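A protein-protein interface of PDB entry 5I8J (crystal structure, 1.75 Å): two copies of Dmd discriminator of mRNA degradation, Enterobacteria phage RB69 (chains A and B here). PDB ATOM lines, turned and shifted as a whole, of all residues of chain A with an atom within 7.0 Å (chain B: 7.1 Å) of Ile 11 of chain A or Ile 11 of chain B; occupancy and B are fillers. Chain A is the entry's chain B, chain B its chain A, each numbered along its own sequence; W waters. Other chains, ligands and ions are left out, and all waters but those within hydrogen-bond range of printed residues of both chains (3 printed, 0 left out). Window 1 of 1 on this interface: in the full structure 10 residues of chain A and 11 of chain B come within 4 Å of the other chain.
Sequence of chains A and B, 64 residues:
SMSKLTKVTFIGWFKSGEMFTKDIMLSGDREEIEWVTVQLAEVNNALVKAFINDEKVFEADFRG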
ATOM      1  N   THR A   9     -14.918   5.035 -13.916  1.00  0.00           N
ATOM      2  CA  THR A   9     -13.758   5.051 -14.797  1.00  0.00           C
ATOM      3  C   THR A   9     -13.530   6.464 -15.300  1.00  0.00           C
ATOM      4  O   THR A   9     -14.397   7.027 -15.931  1.00  0.00           O
ATOM      5  CB  THR A   9     -13.948   4.114 -16.000  1.00  0.00           C
ATOM      6  OG1 THR A   9     -14.094   2.771 -15.532  1.00  0.00           O
ATOM      7  CG2 THR A   9     -12.753   4.202 -16.958  1.00  0.00           C
ATOM      8  N   PHE A  10     -12.372   7.032 -15.000  1.00  0.00           N
ATOM      9  CA  PHE A  10     -12.007   8.361 -15.468  1.00  0.00           C
ATOM     10  C   PHE A  10     -11.009   8.258 -16.605  1.00  0.00           C
ATOM     11  O   PHE A  10     -10.069   7.470 -16.535  1.00  0.00           O
ATOM     12  CB  PHE A  10     -11.408   9.182 -14.329  1.00  0.00           C
ATOM     13  CG  PHE A  10     -12.380   9.480 -13.224  1.00  0.00           C
ATOM     14  CD1 PHE A  10     -13.192  10.607 -13.288  1.00  0.00           C
ATOM     15  CD2 PHE A  10     -12.495   8.628 -12.127  1.00  0.00           C
ATOM     16  CE1 PHE A  10     -14.097  10.883 -12.269  1.00  0.00           C
ATOM     17  CE2 PHE A  10     -13.396   8.901 -11.115  1.00  0.00           C
ATOM     18  CZ  PHE A  10     -14.193  10.034 -11.183  1.00  0.00           C
ATOM     19  N   ILE A  11     -11.231   9.037 -17.660  1.00  0.00           N
ATOM     20  CA  ILE A  11     -10.242   9.204 -18.716  1.00  0.00           C
ATOM     21  C   ILE A  11      -9.820  10.662 -18.735  1.00  0.00           C
ATOM     22  O   ILE A  11     -10.667  11.542 -18.665  1.00  0.00           O
ATOM     23  CB  ILE A  11     -10.775   8.863 -20.102  1.00  0.00           C
ATOM     24  CG1 ILE A  11     -11.573   7.571 -20.106  1.00  0.00           C
ATOM     25  CG2 ILE A  11      -9.631   8.809 -21.123  1.00  0.00           C
ATOM     26  CD1 ILE A  11     -12.206   7.374 -21.431  1.00  0.00           C
ATOM     27  N   GLY A  12      -8.522  10.915 -18.838  1.00  0.00           N
ATOM     28  CA  GLY A  12      -8.020  12.275 -18.865  1.00  0.00           C
ATOM     29  C   GLY A  12      -7.071  12.529 -20.022  1.00  0.00           C
ATOM     30  O   GLY A  12      -6.396  11.615 -20.492  1.00  0.00           O
ATOM     31  N   TRP A  13      -7.044  13.777 -20.472  1.00  0.00           N
ATOM     32  CA  TRP A  13      -6.152  14.262 -21.522  1.00  0.00           C
ATOM     33  C   TRP A  13      -5.389  15.462 -20.981  1.00  0.00           C
ATOM     34  O   TRP A  13      -6.006  16.468 -20.612  1.00  0.00           O
ATOM     35  CB  TRP A  13      -6.931  14.689 -22.769  1.00  0.00           C
ATOM     36  CG  TRP A  13      -7.565  13.576 -23.563  1.00  0.00           C
ATOM     37  CD1 TRP A  13      -7.092  13.028 -24.727  1.00  0.00           C
ATOM     38  CD2 TRP A  13      -8.804  12.912 -23.281  1.00  0.00           C
ATOM     39  NE1 TRP A  13      -7.951  12.049 -25.172  1.00  0.00           N
ATOM     40  CE2 TRP A  13      -9.005  11.956 -24.306  1.00  0.00           C
ATOM     41  CE3 TRP A  13      -9.750  13.015 -22.256  1.00  0.00           C
ATOM     42  CZ2 TRP A  13     -10.118  11.118 -24.329  1.00  0.00           C
ATOM     43  CZ3 TRP A  13     -10.859  12.175 -22.288  1.00  0.00           C
ATOM     44  CH2 TRP A  13     -11.031  11.240 -23.319  1.00  0.00           C
ATOM     45  N   MET A  19      -2.555  10.923 -22.515  1.00  0.00           N
ATOM     46  CA  MET A  19      -3.754  10.493 -21.804  1.00  0.00           C
ATOM     47  C   MET A  19      -3.450   9.741 -20.506  1.00  0.00           C
ATOM     48  O   MET A  19      -2.352   9.225 -20.312  1.00  0.00           O
ATOM     49  CB  MET A  19      -4.615   9.626 -22.739  1.00  0.00           C
ATOM     50  CG  MET A  19      -5.134  10.404 -23.953  1.00  0.00           C
ATOM     51  SD  MET A  19      -5.955   9.424 -25.240  1.00  0.00           S
ATOM     52  CE  MET A  19      -7.357   8.781 -24.315  1.00  0.00           C
ATOM     53  N   PHE A  20      -4.430   9.697 -19.606  1.00  0.00           N
ATOM     54  CA  PHE A  20      -4.348   8.844 -18.424  1.00  0.00           C
ATOM     55  C   PHE A  20      -5.727   8.269 -18.144  1.00  0.00           C
ATOM     56  O   PHE A  20      -6.718   8.790 -18.622  1.00  0.00           O
ATOM     57  CB  PHE A  20      -3.801   9.615 -17.215  1.00  0.00           C
ATOM     58  CG  PHE A  20      -4.665  10.769 -16.754  1.00  0.00           C
ATOM     59  CD1 PHE A  20      -4.522  12.030 -17.313  1.00  0.00           C
ATOM     60  CD2 PHE A  20      -5.564  10.605 -15.708  1.00  0.00           C
ATOM     61  CE1 PHE A  20      -5.283  13.100 -16.864  1.00  0.00           C
ATOM     62  CE2 PHE A  20      -6.327  11.670 -15.257  1.00  0.00           C
ATOM     63  CZ  PHE A  20      -6.186  12.917 -15.841  1.00  0.00           C
ATOM     64  N   THR A  21      -5.797   7.166 -17.422  1.00  0.00           N
ATOM     65  CA  THR A  21      -7.105   6.600 -17.125  1.00  0.00           C
ATOM     66  C   THR A  21      -7.032   5.846 -15.811  1.00  0.00           C
ATOM     67  O   THR A  21      -6.075   5.101 -15.563  1.00  0.00           O
ATOM     68  CB  THR A  21      -7.617   5.686 -18.284  1.00  0.00           C
ATOM     69  OG1 THR A  21      -8.949   5.232 -18.006  1.00  0.00           O
ATOM     70  CG2 THR A  21      -6.713   4.483 -18.507  1.00  0.00           C
ATOM     71  N   LYS A  22      -8.065   6.056 -14.989  1.00  0.00           N
ATOM     72  CA  LYS A  22      -8.080   5.782 -13.554  1.00  0.00           C
ATOM     73  C   LYS A  22      -9.383   5.067 -13.211  1.00  0.00           C
ATOM     74  O   LYS A  22     -10.426   5.501 -13.661  1.00  0.00           O
ATOM     75  CB  LYS A  22      -7.990   7.108 -12.788  1.00  0.00           C
ATOM     76  CG  LYS A  22      -7.343   7.076 -11.416  1.00  0.00           C
ATOM     77  CD  LYS A  22      -6.635   8.402 -11.189  1.00  0.00           C
ATOM     78  CE  LYS A  22      -6.080   8.535  -9.783  1.00  0.00           C
ATOM     79  NZ  LYS A  22      -4.740   7.916  -9.643  1.00  0.00           N
ATOM     80  N   ASP A  23      -9.339   3.990 -12.433  1.00  0.00           N
ATOM     81  CA  ASP A  23     -10.561   3.340 -11.951  1.00  0.00           C
ATOM     82  C   ASP A  23     -10.675   3.586 -10.451  1.00  0.00           C
ATOM     83  O   ASP A  23      -9.836   3.107  -9.694  1.00  0.00           O
ATOM     84  CB  ASP A  23     -10.537   1.825 -12.223  1.00  0.00           C
ATOM     85  CG  ASP A  23     -11.486   1.390 -13.332  1.00  0.00           C
ATOM     86  OD1 ASP A  23     -12.077   2.251 -14.020  1.00  0.00           O
ATOM     87  OD2 ASP A  23     -11.607   0.160 -13.550  1.00  0.00           O
ATOM     88  N   LEU A  47      -8.354  17.686 -19.341  1.00  0.00           N
ATOM     89  CA  LEU A  47      -9.732  17.362 -19.665  1.00  0.00           C
ATOM     90  C   LEU A  47     -10.004  15.994 -19.050  1.00  0.00           C
ATOM     91  O   LEU A  47      -9.256  15.058 -19.279  1.00  0.00           O
ATOM     92  CB  LEU A  47      -9.962  17.334 -21.177  1.00  0.00           C
ATOM     93  CG  LEU A  47     -11.251  16.674 -21.663  1.00  0.00           C
ATOM     94  CD1 LEU A  47     -12.460  17.550 -21.331  1.00  0.00           C
ATOM     95  CD2 LEU A  47     -11.164  16.374 -23.170  1.00  0.00           C
ATOM     96  N   VAL A  48     -11.051  15.880 -18.251  1.00  0.00           N
ATOM     97  CA  VAL A  48     -11.374  14.608 -17.620  1.00  0.00           C
ATOM     98  C   VAL A  48     -12.839  14.280 -17.853  1.00  0.00           C
ATOM     99  O   VAL A  48     -13.709  15.138 -17.707  1.00  0.00           O
ATOM    100  CB  VAL A  48     -11.063  14.617 -16.107  1.00  0.00           C
ATOM    101  CG1 VAL A  48     -11.546  13.326 -15.452  1.00  0.00           C
ATOM    102  CG2 VAL A  48      -9.560  14.793 -15.872  1.00  0.00           C
ATOM    103  N   LYS A  49     -13.083  13.036 -18.262  1.00  0.00           N
ATOM    104  CA  LYS A  49     -14.417  12.490 -18.455  1.00  0.00           C
ATOM    105  C   LYS A  49     -14.628  11.358 -17.473  1.00  0.00           C
ATOM    106  O   LYS A  49     -13.730  10.537 -17.263  1.00  0.00           O
ATOM    107  CB  LYS A  49     -14.606  11.967 -19.881  1.00  0.00           C
ATOM    108  CG  LYS A  49     -14.414  13.014 -20.964  1.00  0.00           C
ATOM    109  CD  LYS A  49     -14.548  12.395 -22.344  1.00  0.00           C
ATOM    110  CE  LYS A  49     -14.256  13.425 -23.427  1.00  0.00           C
ATOM    111  NZ  LYS A  49     -14.295  12.823 -24.786  1.00  0.00           N
ATOM    112  N   ALA A  50     -15.814  11.330 -16.871  1.00  0.00           N
ATOM    113  CA  ALA A  50     -16.186  10.301 -15.913  1.00  0.00           C
ATOM    114  C   ALA A  50     -17.210   9.376 -16.550  1.00  0.00           C
ATOM    115  O   ALA A  50     -18.221   9.836 -17.076  1.00  0.00           O
ATOM    116  CB  ALA A  50     -16.756  10.926 -14.630  1.00  0.00           C
ATOM    117  N   PHE A  51     -16.930   8.078 -16.496  1.00  0.00           N
ATOM    118  CA  PHE A  51     -17.797   7.046 -17.045  1.00  0.00           C
ATOM    119  C   PHE A  51     -18.306   6.133 -15.936  1.00  0.00           C
ATOM    120  O   PHE A  51     -17.523   5.616 -15.136  1.00  0.00           O
ATOM    121  CB  PHE A  51     -17.065   6.199 -18.093  1.00  0.00           C
ATOM    122  CG  PHE A  51     -16.751   6.941 -19.357  1.00  0.00           C
ATOM    123  CD1 PHE A  51     -15.612   7.716 -19.450  1.00  0.00           C
ATOM    124  CD2 PHE A  51     -17.598   6.865 -20.448  1.00  0.00           C
ATOM    125  CE1 PHE A  51     -15.322   8.414 -20.623  1.00  0.00           C
ATOM    126  CE2 PHE A  51     -17.313   7.553 -21.616  1.00  0.00           C
ATOM    127  CZ  PHE A  51     -16.176   8.327 -21.700  1.00  0.00           C
ATOM    128  N   ASP A  54     -20.061   2.568 -18.456  1.00  0.00           N
ATOM    129  CA  ASP A  54     -19.667   2.968 -19.804  1.00  0.00           C
ATOM    130  C   ASP A  54     -20.479   4.120 -20.383  1.00  0.00           C
ATOM    131  O   ASP A  54     -20.439   4.369 -21.586  1.00  0.00           O
ATOM    132  CB  ASP A  54     -19.721   1.766 -20.754  1.00  0.00           C
ATOM    133  CG  ASP A  54     -18.741   0.680 -20.368  1.00  0.00           C
ATOM    134  OD1 ASP A  54     -17.720   1.008 -19.737  1.00  0.00           O
ATOM    135  OD2 ASP A  54     -18.990  -0.498 -20.696  1.00  0.00           O
ATOM    136  N   THR B   9     -11.794   6.423 -29.083  1.00  0.00           N
ATOM    137  CA  THR B   9     -11.104   6.304 -27.806  1.00  0.00           C
ATOM    138  C   THR B   9     -11.211   4.859 -27.326  1.00  0.00           C
ATOM    139  O   THR B   9     -12.307   4.339 -27.174  1.00  0.00           O
ATOM    140  CB  THR B   9     -11.698   7.244 -26.739  1.00  0.00           C
ATOM    141  OG1 THR B   9     -11.589   8.613 -27.177  1.00  0.00           O
ATOM    142  CG2 THR B   9     -10.966   7.068 -25.413  1.00  0.00           C
ATOM    143  N   PHE B  10     -10.070   4.224 -27.116  1.00  0.00           N
ATOM    144  CA  PHE B  10     -10.008   2.854 -26.631  1.00  0.00           C
ATOM    145  C   PHE B  10      -9.618   2.871 -25.168  1.00  0.00           C
ATOM    146  O   PHE B  10      -8.675   3.576 -24.774  1.00  0.00           O
ATOM    147  CB  PHE B  10      -8.999   2.026 -27.435  1.00  0.00           C
ATOM    148  CG  PHE B  10      -9.396   1.799 -28.864  1.00  0.00           C
ATOM    149  CD1 PHE B  10     -10.152   0.688 -29.222  1.00  0.00           C
ATOM    150  CD2 PHE B  10      -9.022   2.695 -29.849  1.00  0.00           C
ATOM    151  CE1 PHE B  10     -10.517   0.477 -30.533  1.00  0.00           C
ATOM    152  CE2 PHE B  10      -9.388   2.492 -31.169  1.00  0.00           C
ATOM    153  CZ  PHE B  10     -10.136   1.387 -31.514  1.00  0.00           C
ATOM    154  N   ILE B  11     -10.351   2.108 -24.362  1.00  0.00           N
ATOM    155  CA  ILE B  11     -10.005   1.935 -22.959  1.00  0.00           C
ATOM    156  C   ILE B  11      -9.787   0.464 -22.700  1.00  0.00           C
ATOM    157  O   ILE B  11     -10.622  -0.351 -23.049  1.00  0.00           O
ATOM    158  CB  ILE B  11     -11.096   2.442 -22.016  1.00  0.00           C
ATOM    159  CG1 ILE B  11     -11.553   3.841 -22.423  1.00  0.00           C
ATOM    160  CG2 ILE B  11     -10.586   2.430 -20.583  1.00  0.00           C
ATOM    161  CD1 ILE B  11     -12.862   4.187 -21.772  1.00  0.00           C
ATOM    162  N   GLY B  12      -8.650   0.132 -22.107  1.00  0.00           N
ATOM    163  CA  GLY B  12      -8.261  -1.252 -21.898  1.00  0.00           C
ATOM    164  C   GLY B  12      -8.001  -1.564 -20.434  1.00  0.00           C
ATOM    165  O   GLY B  12      -7.493  -0.719 -19.685  1.00  0.00           O
ATOM    166  N   TRP B  13      -8.394  -2.771 -20.034  1.00  0.00           N
ATOM    167  CA  TRP B  13      -8.068  -3.347 -18.734  1.00  0.00           C
ATOM    168  C   TRP B  13      -7.251  -4.618 -18.897  1.00  0.00           C
ATOM    169  O   TRP B  13      -7.715  -5.584 -19.517  1.00  0.00           O
ATOM    170  CB  TRP B  13      -9.332  -3.688 -17.943  1.00  0.00           C
ATOM    171  CG  TRP B  13     -10.093  -2.519 -17.429  1.00  0.00           C
ATOM    172  CD1 TRP B  13     -10.077  -2.027 -16.151  1.00  0.00           C
ATOM    173  CD2 TRP B  13     -11.028  -1.716 -18.161  1.00  0.00           C
ATOM    174  NE1 TRP B  13     -10.932  -0.949 -16.055  1.00  0.00           N
ATOM    175  CE2 TRP B  13     -11.527  -0.742 -17.267  1.00  0.00           C
ATOM    176  CE3 TRP B  13     -11.480  -1.718 -19.482  1.00  0.00           C
ATOM    177  CZ2 TRP B  13     -12.457   0.225 -17.659  1.00  0.00           C
ATOM    178  CZ3 TRP B  13     -12.411  -0.754 -19.867  1.00  0.00           C
ATOM    179  CH2 TRP B  13     -12.886   0.201 -18.952  1.00  0.00           C
ATOM    180  N   MET B  19      -4.661  -0.404 -16.351  1.00  0.00           N
ATOM    181  CA  MET B  19      -5.406   0.095 -17.499  1.00  0.00           C
ATOM    182  C   MET B  19      -4.510   0.749 -18.526  1.00  0.00           C
ATOM    183  O   MET B  19      -3.375   1.130 -18.220  1.00  0.00           O
ATOM    184  CB  MET B  19      -6.477   1.087 -17.031  1.00  0.00           C
ATOM    185  CG  MET B  19      -7.509   0.418 -16.145  1.00  0.00           C
ATOM    186  SD  MET B  19      -8.581   1.596 -15.294  1.00  0.00           S
ATOM    187  CE  MET B  19      -9.380   2.348 -16.671  1.00  0.00           C
ATOM    188  N   PHE B  20      -5.019   0.861 -19.750  1.00  0.00           N
ATOM    189  CA  PHE B  20      -4.378   1.688 -20.766  1.00  0.00           C
ATOM    190  C   PHE B  20      -5.443   2.383 -21.593  1.00  0.00           C
ATOM    191  O   PHE B  20      -6.592   1.975 -21.596  1.00  0.00           O
ATOM    192  CB  PHE B  20      -3.444   0.860 -21.663  1.00  0.00           C
ATOM    193  CG  PHE B  20      -4.130  -0.223 -22.447  1.00  0.00           C
ATOM    194  CD1 PHE B  20      -4.351  -1.474 -21.884  1.00  0.00           C
ATOM    195  CD2 PHE B  20      -4.524  -0.003 -23.759  1.00  0.00           C
ATOM    196  CE1 PHE B  20      -4.974  -2.476 -22.608  1.00  0.00           C
ATOM    197  CE2 PHE B  20      -5.146  -1.008 -24.490  1.00  0.00           C
ATOM    198  CZ  PHE B  20      -5.368  -2.237 -23.919  1.00  0.00           C
ATOM    199  N   THR B  21      -5.077   3.454 -22.281  1.00  0.00           N
ATOM    200  CA  THR B  21      -6.069   4.158 -23.084  1.00  0.00           C
ATOM    201  C   THR B  21      -5.368   4.832 -24.263  1.00  0.00           C
ATOM    202  O   THR B  21      -4.210   5.220 -24.152  1.00  0.00           O
ATOM    203  CB  THR B  21      -6.862   5.175 -22.226  1.00  0.00           C
ATOM    204  OG1 THR B  21      -7.931   5.732 -22.998  1.00  0.00           O
ATOM    205  CG2 THR B  21      -5.956   6.293 -21.714  1.00  0.00           C
ATOM    206  N   LYS B  22      -6.055   4.899 -25.404  1.00  0.00           N
ATOM    207  CA  LYS B  22      -5.481   5.509 -26.605  1.00  0.00           C
ATOM    208  C   LYS B  22      -6.554   6.165 -27.435  1.00  0.00           C
ATOM    209  O   LYS B  22      -7.652   5.646 -27.510  1.00  0.00           O
ATOM    210  CB  LYS B  22      -4.785   4.466 -27.492  1.00  0.00           C
ATOM    211  CG  LYS B  22      -3.644   3.705 -26.885  1.00  0.00           C
ATOM    212  CD  LYS B  22      -3.017   2.800 -27.926  1.00  0.00           C
ATOM    213  CE  LYS B  22      -2.320   3.612 -29.000  1.00  0.00           C
ATOM    214  NZ  LYS B  22      -1.410   2.746 -29.810  1.00  0.00           N
ATOM    215  N   ASP B  23      -6.222   7.279 -28.090  1.00  0.00           N
ATOM    216  CA  ASP B  23      -7.066   7.843 -29.143  1.00  0.00           C
ATOM    217  C   ASP B  23      -6.475   7.456 -30.486  1.00  0.00           C
ATOM    218  O   ASP B  23      -5.300   7.708 -30.728  1.00  0.00           O
ATOM    219  CB  ASP B  23      -7.147   9.369 -29.045  1.00  0.00           C
ATOM    220  CG  ASP B  23      -8.201   9.835 -28.071  1.00  0.00           C
ATOM    221  OD1 ASP B  23      -8.909   8.978 -27.512  1.00  0.00           O
ATOM    222  OD2 ASP B  23      -8.341  11.058 -27.889  1.00  0.00           O
ATOM    223  N   LEU B  40      -6.277  -5.190 -30.508  1.00  0.00           N
ATOM    224  CA  LEU B  40      -5.800  -4.543 -29.291  1.00  0.00           C
ATOM    225  C   LEU B  40      -6.026  -5.433 -28.077  1.00  0.00           C
ATOM    226  O   LEU B  40      -5.141  -5.596 -27.233  1.00  0.00           O
ATOM    227  CB  LEU B  40      -6.509  -3.202 -29.081  1.00  0.00           C
ATOM    228  CG  LEU B  40      -5.823  -1.933 -29.570  1.00  0.00           C
ATOM    229  CD1 LEU B  40      -6.705  -0.734 -29.240  1.00  0.00           C
ATOM    230  CD2 LEU B  40      -4.445  -1.793 -28.924  1.00  0.00           C
ATOM    231  N   LEU B  47      -9.330  -6.635 -21.758  1.00  0.00           N
ATOM    232  CA  LEU B  47     -10.662  -6.182 -22.122  1.00  0.00           C
ATOM    233  C   LEU B  47     -10.481  -4.821 -22.759  1.00  0.00           C
ATOM    234  O   LEU B  47      -9.867  -3.950 -22.160  1.00  0.00           O
ATOM    235  CB  LEU B  47     -11.572  -6.086 -20.894  1.00  0.00           C
ATOM    236  CG  LEU B  47     -12.856  -5.265 -21.040  1.00  0.00           C
ATOM    237  CD1 LEU B  47     -13.824  -5.937 -22.006  1.00  0.00           C
ATOM    238  CD2 LEU B  47     -13.513  -5.042 -19.685  1.00  0.00           C
ATOM    239  N   VAL B  48     -10.976  -4.631 -23.975  1.00  0.00           N
ATOM    240  CA  VAL B  48     -10.866  -3.314 -24.611  1.00  0.00           C
ATOM    241  C   VAL B  48     -12.233  -2.854 -25.077  1.00  0.00           C
ATOM    242  O   VAL B  48     -12.971  -3.628 -25.692  1.00  0.00           O
ATOM    243  CB  VAL B  48      -9.887  -3.334 -25.809  1.00  0.00           C
ATOM    244  CG1 VAL B  48      -9.831  -1.945 -26.488  1.00  0.00           C
ATOM    245  CG2 VAL B  48      -8.503  -3.757 -25.353  1.00  0.00           C
ATOM    246  N   LYS B  49     -12.572  -1.603 -24.749  1.00  0.00           N
ATOM    247  CA  LYS B  49     -13.809  -0.967 -25.181  1.00  0.00           C
ATOM    248  C   LYS B  49     -13.483   0.157 -26.146  1.00  0.00           C
ATOM    249  O   LYS B  49     -12.549   0.930 -25.903  1.00  0.00           O
ATOM    250  CB  LYS B  49     -14.595  -0.402 -23.998  1.00  0.00           C
ATOM    251  CG  LYS B  49     -14.914  -1.405 -22.903  1.00  0.00           C
ATOM    252  CD  LYS B  49     -15.460  -0.669 -21.665  1.00  0.00           C
ATOM    253  CE  LYS B  49     -15.650  -1.608 -20.484  1.00  0.00           C
ATOM    254  NZ  LYS B  49     -16.911  -2.376 -20.554  1.00  0.00           N
ATOM    255  N   ALA B  50     -14.256   0.243 -27.228  1.00  0.00           N
ATOM    256  CA  ALA B  50     -14.121   1.333 -28.198  1.00  0.00           C
ATOM    257  C   ALA B  50     -15.269   2.338 -28.032  1.00  0.00           C
ATOM    258  O   ALA B  50     -16.435   1.965 -27.978  1.00  0.00           O
ATOM    259  CB  ALA B  50     -14.087   0.776 -29.628  1.00  0.00           C
ATOM    260  N   PHE B  51     -14.914   3.614 -27.946  1.00  0.00           N
ATOM    261  CA  PHE B  51     -15.855   4.703 -27.764  1.00  0.00           C
ATOM    262  C   PHE B  51     -15.766   5.673 -28.937  1.00  0.00           C
ATOM    263  O   PHE B  51     -14.671   6.050 -29.346  1.00  0.00           O
ATOM    264  CB  PHE B  51     -15.572   5.466 -26.460  1.00  0.00           C
ATOM    265  CG  PHE B  51     -15.958   4.723 -25.207  1.00  0.00           C
ATOM    266  CD1 PHE B  51     -15.123   3.749 -24.664  1.00  0.00           C
ATOM    267  CD2 PHE B  51     -17.144   5.028 -24.548  1.00  0.00           C
ATOM    268  CE1 PHE B  51     -15.485   3.076 -23.498  1.00  0.00           C
ATOM    269  CE2 PHE B  51     -17.507   4.356 -23.383  1.00  0.00           C
ATOM    270  CZ  PHE B  51     -16.676   3.387 -22.856  1.00  0.00           C
ATOM    271  N   ASP B  54     -18.006   9.547 -27.133  1.00  0.00           N
ATOM    272  CA  ASP B  54     -18.269   9.184 -25.731  1.00  0.00           C
ATOM    273  C   ASP B  54     -19.293   8.056 -25.557  1.00  0.00           C
ATOM    274  O   ASP B  54     -19.777   7.818 -24.457  1.00  0.00           O
ATOM    275  CB  ASP B  54     -18.708  10.420 -24.942  1.00  0.00           C
ATOM    276  CG  ASP B  54     -17.614  11.462 -24.849  1.00  0.00           C
ATOM    277  OD1 ASP B  54     -16.435  11.063 -24.753  1.00  0.00           O
ATOM    278  OD2 ASP B  54     -17.930  12.671 -24.884  1.00  0.00           O
HETATM  279  O   HOH W   1      -3.679   8.509 -27.571  1.00  0.00           O
HETATM  280  O   HOH W   2     -13.140  11.259 -26.239  1.00  0.00           O
HETATM  281  O   HOH W   3     -10.486  12.465 -27.313  1.00  0.00           O
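The side-chain sulfur (SD) of Met 19 of chain B lies close to the side-chain carboxylate (OD2) of Asp 23 of chain A (3.8 Å). OD1 of Asp 54 of chain B is in salt-bridge range of NZ of Lys 49 of chain A, at 2.8 Å. The backbone NH (N) of Asp 23 of chain B sits at hydrogen-bond distance from the side-chain sulfur (SD) of Met 19 of chain A, 3.6 Å away. OD2 of Asp 23 of chain B sits at hydrogen-bond distance from NE1 of Trp 13 of chain A, 2.9 Å away. The side-chain amino group of Lys 49 of chain B lies within salt-bridge range of the side-chain carboxylate of Asp 54 of chain A (2.8 Å). The indole nitrogen (NE1) of Trp 13 of chain B sits at hydrogen-bond distance from the side-chain carboxylate (OD2) of Asp 23 of chain A (2.8 Å).
O of Ile 11 of chain A sits at hydrogen-bond distance from N of Lys 49 of chain A. The backbone NH (N) of Lys 49 of chain B lies within hydrogen-bond range of the backbone carbonyl oxygen (O) of Ile 11 of chain B, 2.9 Å away. O of Leu 47 of chain A lies within hydrogen-bond range of N of Trp 13 of chain A (2.8 Å). O of Phe 10 of chain B is in hydrogen-bond range of OG1 of Thr 21 of chain B (2.9 Å). O of Thr 9 of chain B lies within hydrogen-bond range of N of Phe 51 of chain B. N of Trp 13 of chain B is in hydrogen-bond range of O of Leu 47 of chain B, at 2.8 Å.
Among the printed residues, pairs that only touch across the chains: Thr 9 of chain A with Trp 13 of chain B (3.7 Å), Thr 9 of chain A with Met 19 of chain B (3.9 Å), Ile 11 of chain A with Ile 11 of chain B (3.3 Å), Ile 11 of chain A with Thr 21 of chain B (3.98 Å), Met 19 of chain A with Thr 21 of chain B (3.4 Å), Met 19 of chain A with Lys 22 of chain B (3.97 Å), Thr 21 of chain A with Met 19 of chain B (3.2 Å), Thr 21 of chain A with Phe 20 of chain B (3.9 Å), Thr 21 of chain A with Thr 21 of chain B (3.8 Å), Phe 51 of chain A with Phe 51 of chain B (3.7 Å), Phe 51 of chain A with Asp 54 of chain B (3.8 Å) and Asp 54 of chain A with Phe 51 of chain B (3.4 Å).
Of the printed residues of chain B, Ile 11 of chain A touches Ile 11 and Thr 21. Of the printed residues of chain B, Thr 21 of chain A touches Met 19 (3.2 Å), Phe 20 (3.9 Å) and Thr 21 (3.8 Å). Of the printed residues of chain A, Lys 49 of chain B touches Asp 54.
Printed residues of chain A that touch a printed residue of chain B: Thr 9, Ile 11, Trp 13, Met 19, Thr 21, Asp 23, Lys 49, Phe 51 and Asp 54. Among the printed residues, Asp or Glu carboxylates within 4 Å of a Lys or Arg side-chain nitrogen of the other chain: Lys 49 of chain A with Asp 54 of chain B (2.8 Å) and Asp 54 of chain A with Lys 49 of chain B (2.8 Å).
Thr 9 of chain A touches Trp 13 of chain B, but with the chains exchanged Trp 13 of chain A does not touch Thr 9 of chain B (4.1 Å). Ile 11 of chain A touches Thr 21 of chain B, but with the chains exchanged Thr 21 of chain A does not touch Ile 11 of chain B (4.1 Å). Met 19 of chain A touches Asp 23 of chain B, and with the chains exchanged Asp 23 of chain A touches Met 19 of chain B. Lys 49 of chain A touches Asp 54 of chain B, and with the chains exchanged Asp 54 of chain A touches Lys 49 of chain B. Positions printed for both chains: 9, 10, 11, 12, 13, 19, 20, 21, 22, 23, 47, 48, 49, 50, 51 and 54.
Water W2 bridges NZ of Lys 49 of chain A (2.4 Å) and OG1 of Thr 9 of chain B (3.2 Å). Water W3 bridges the side-chain carboxylate (OD2) of Asp 23 of chain B (2.6 Å) and the indole nitrogen (NE1) of Trp 13 of chain A (3.3 Å). Water W1 bridges N of Asp 23 of chain B (2.9 Å) and SD of Met 19 of chain A (3.4 Å).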
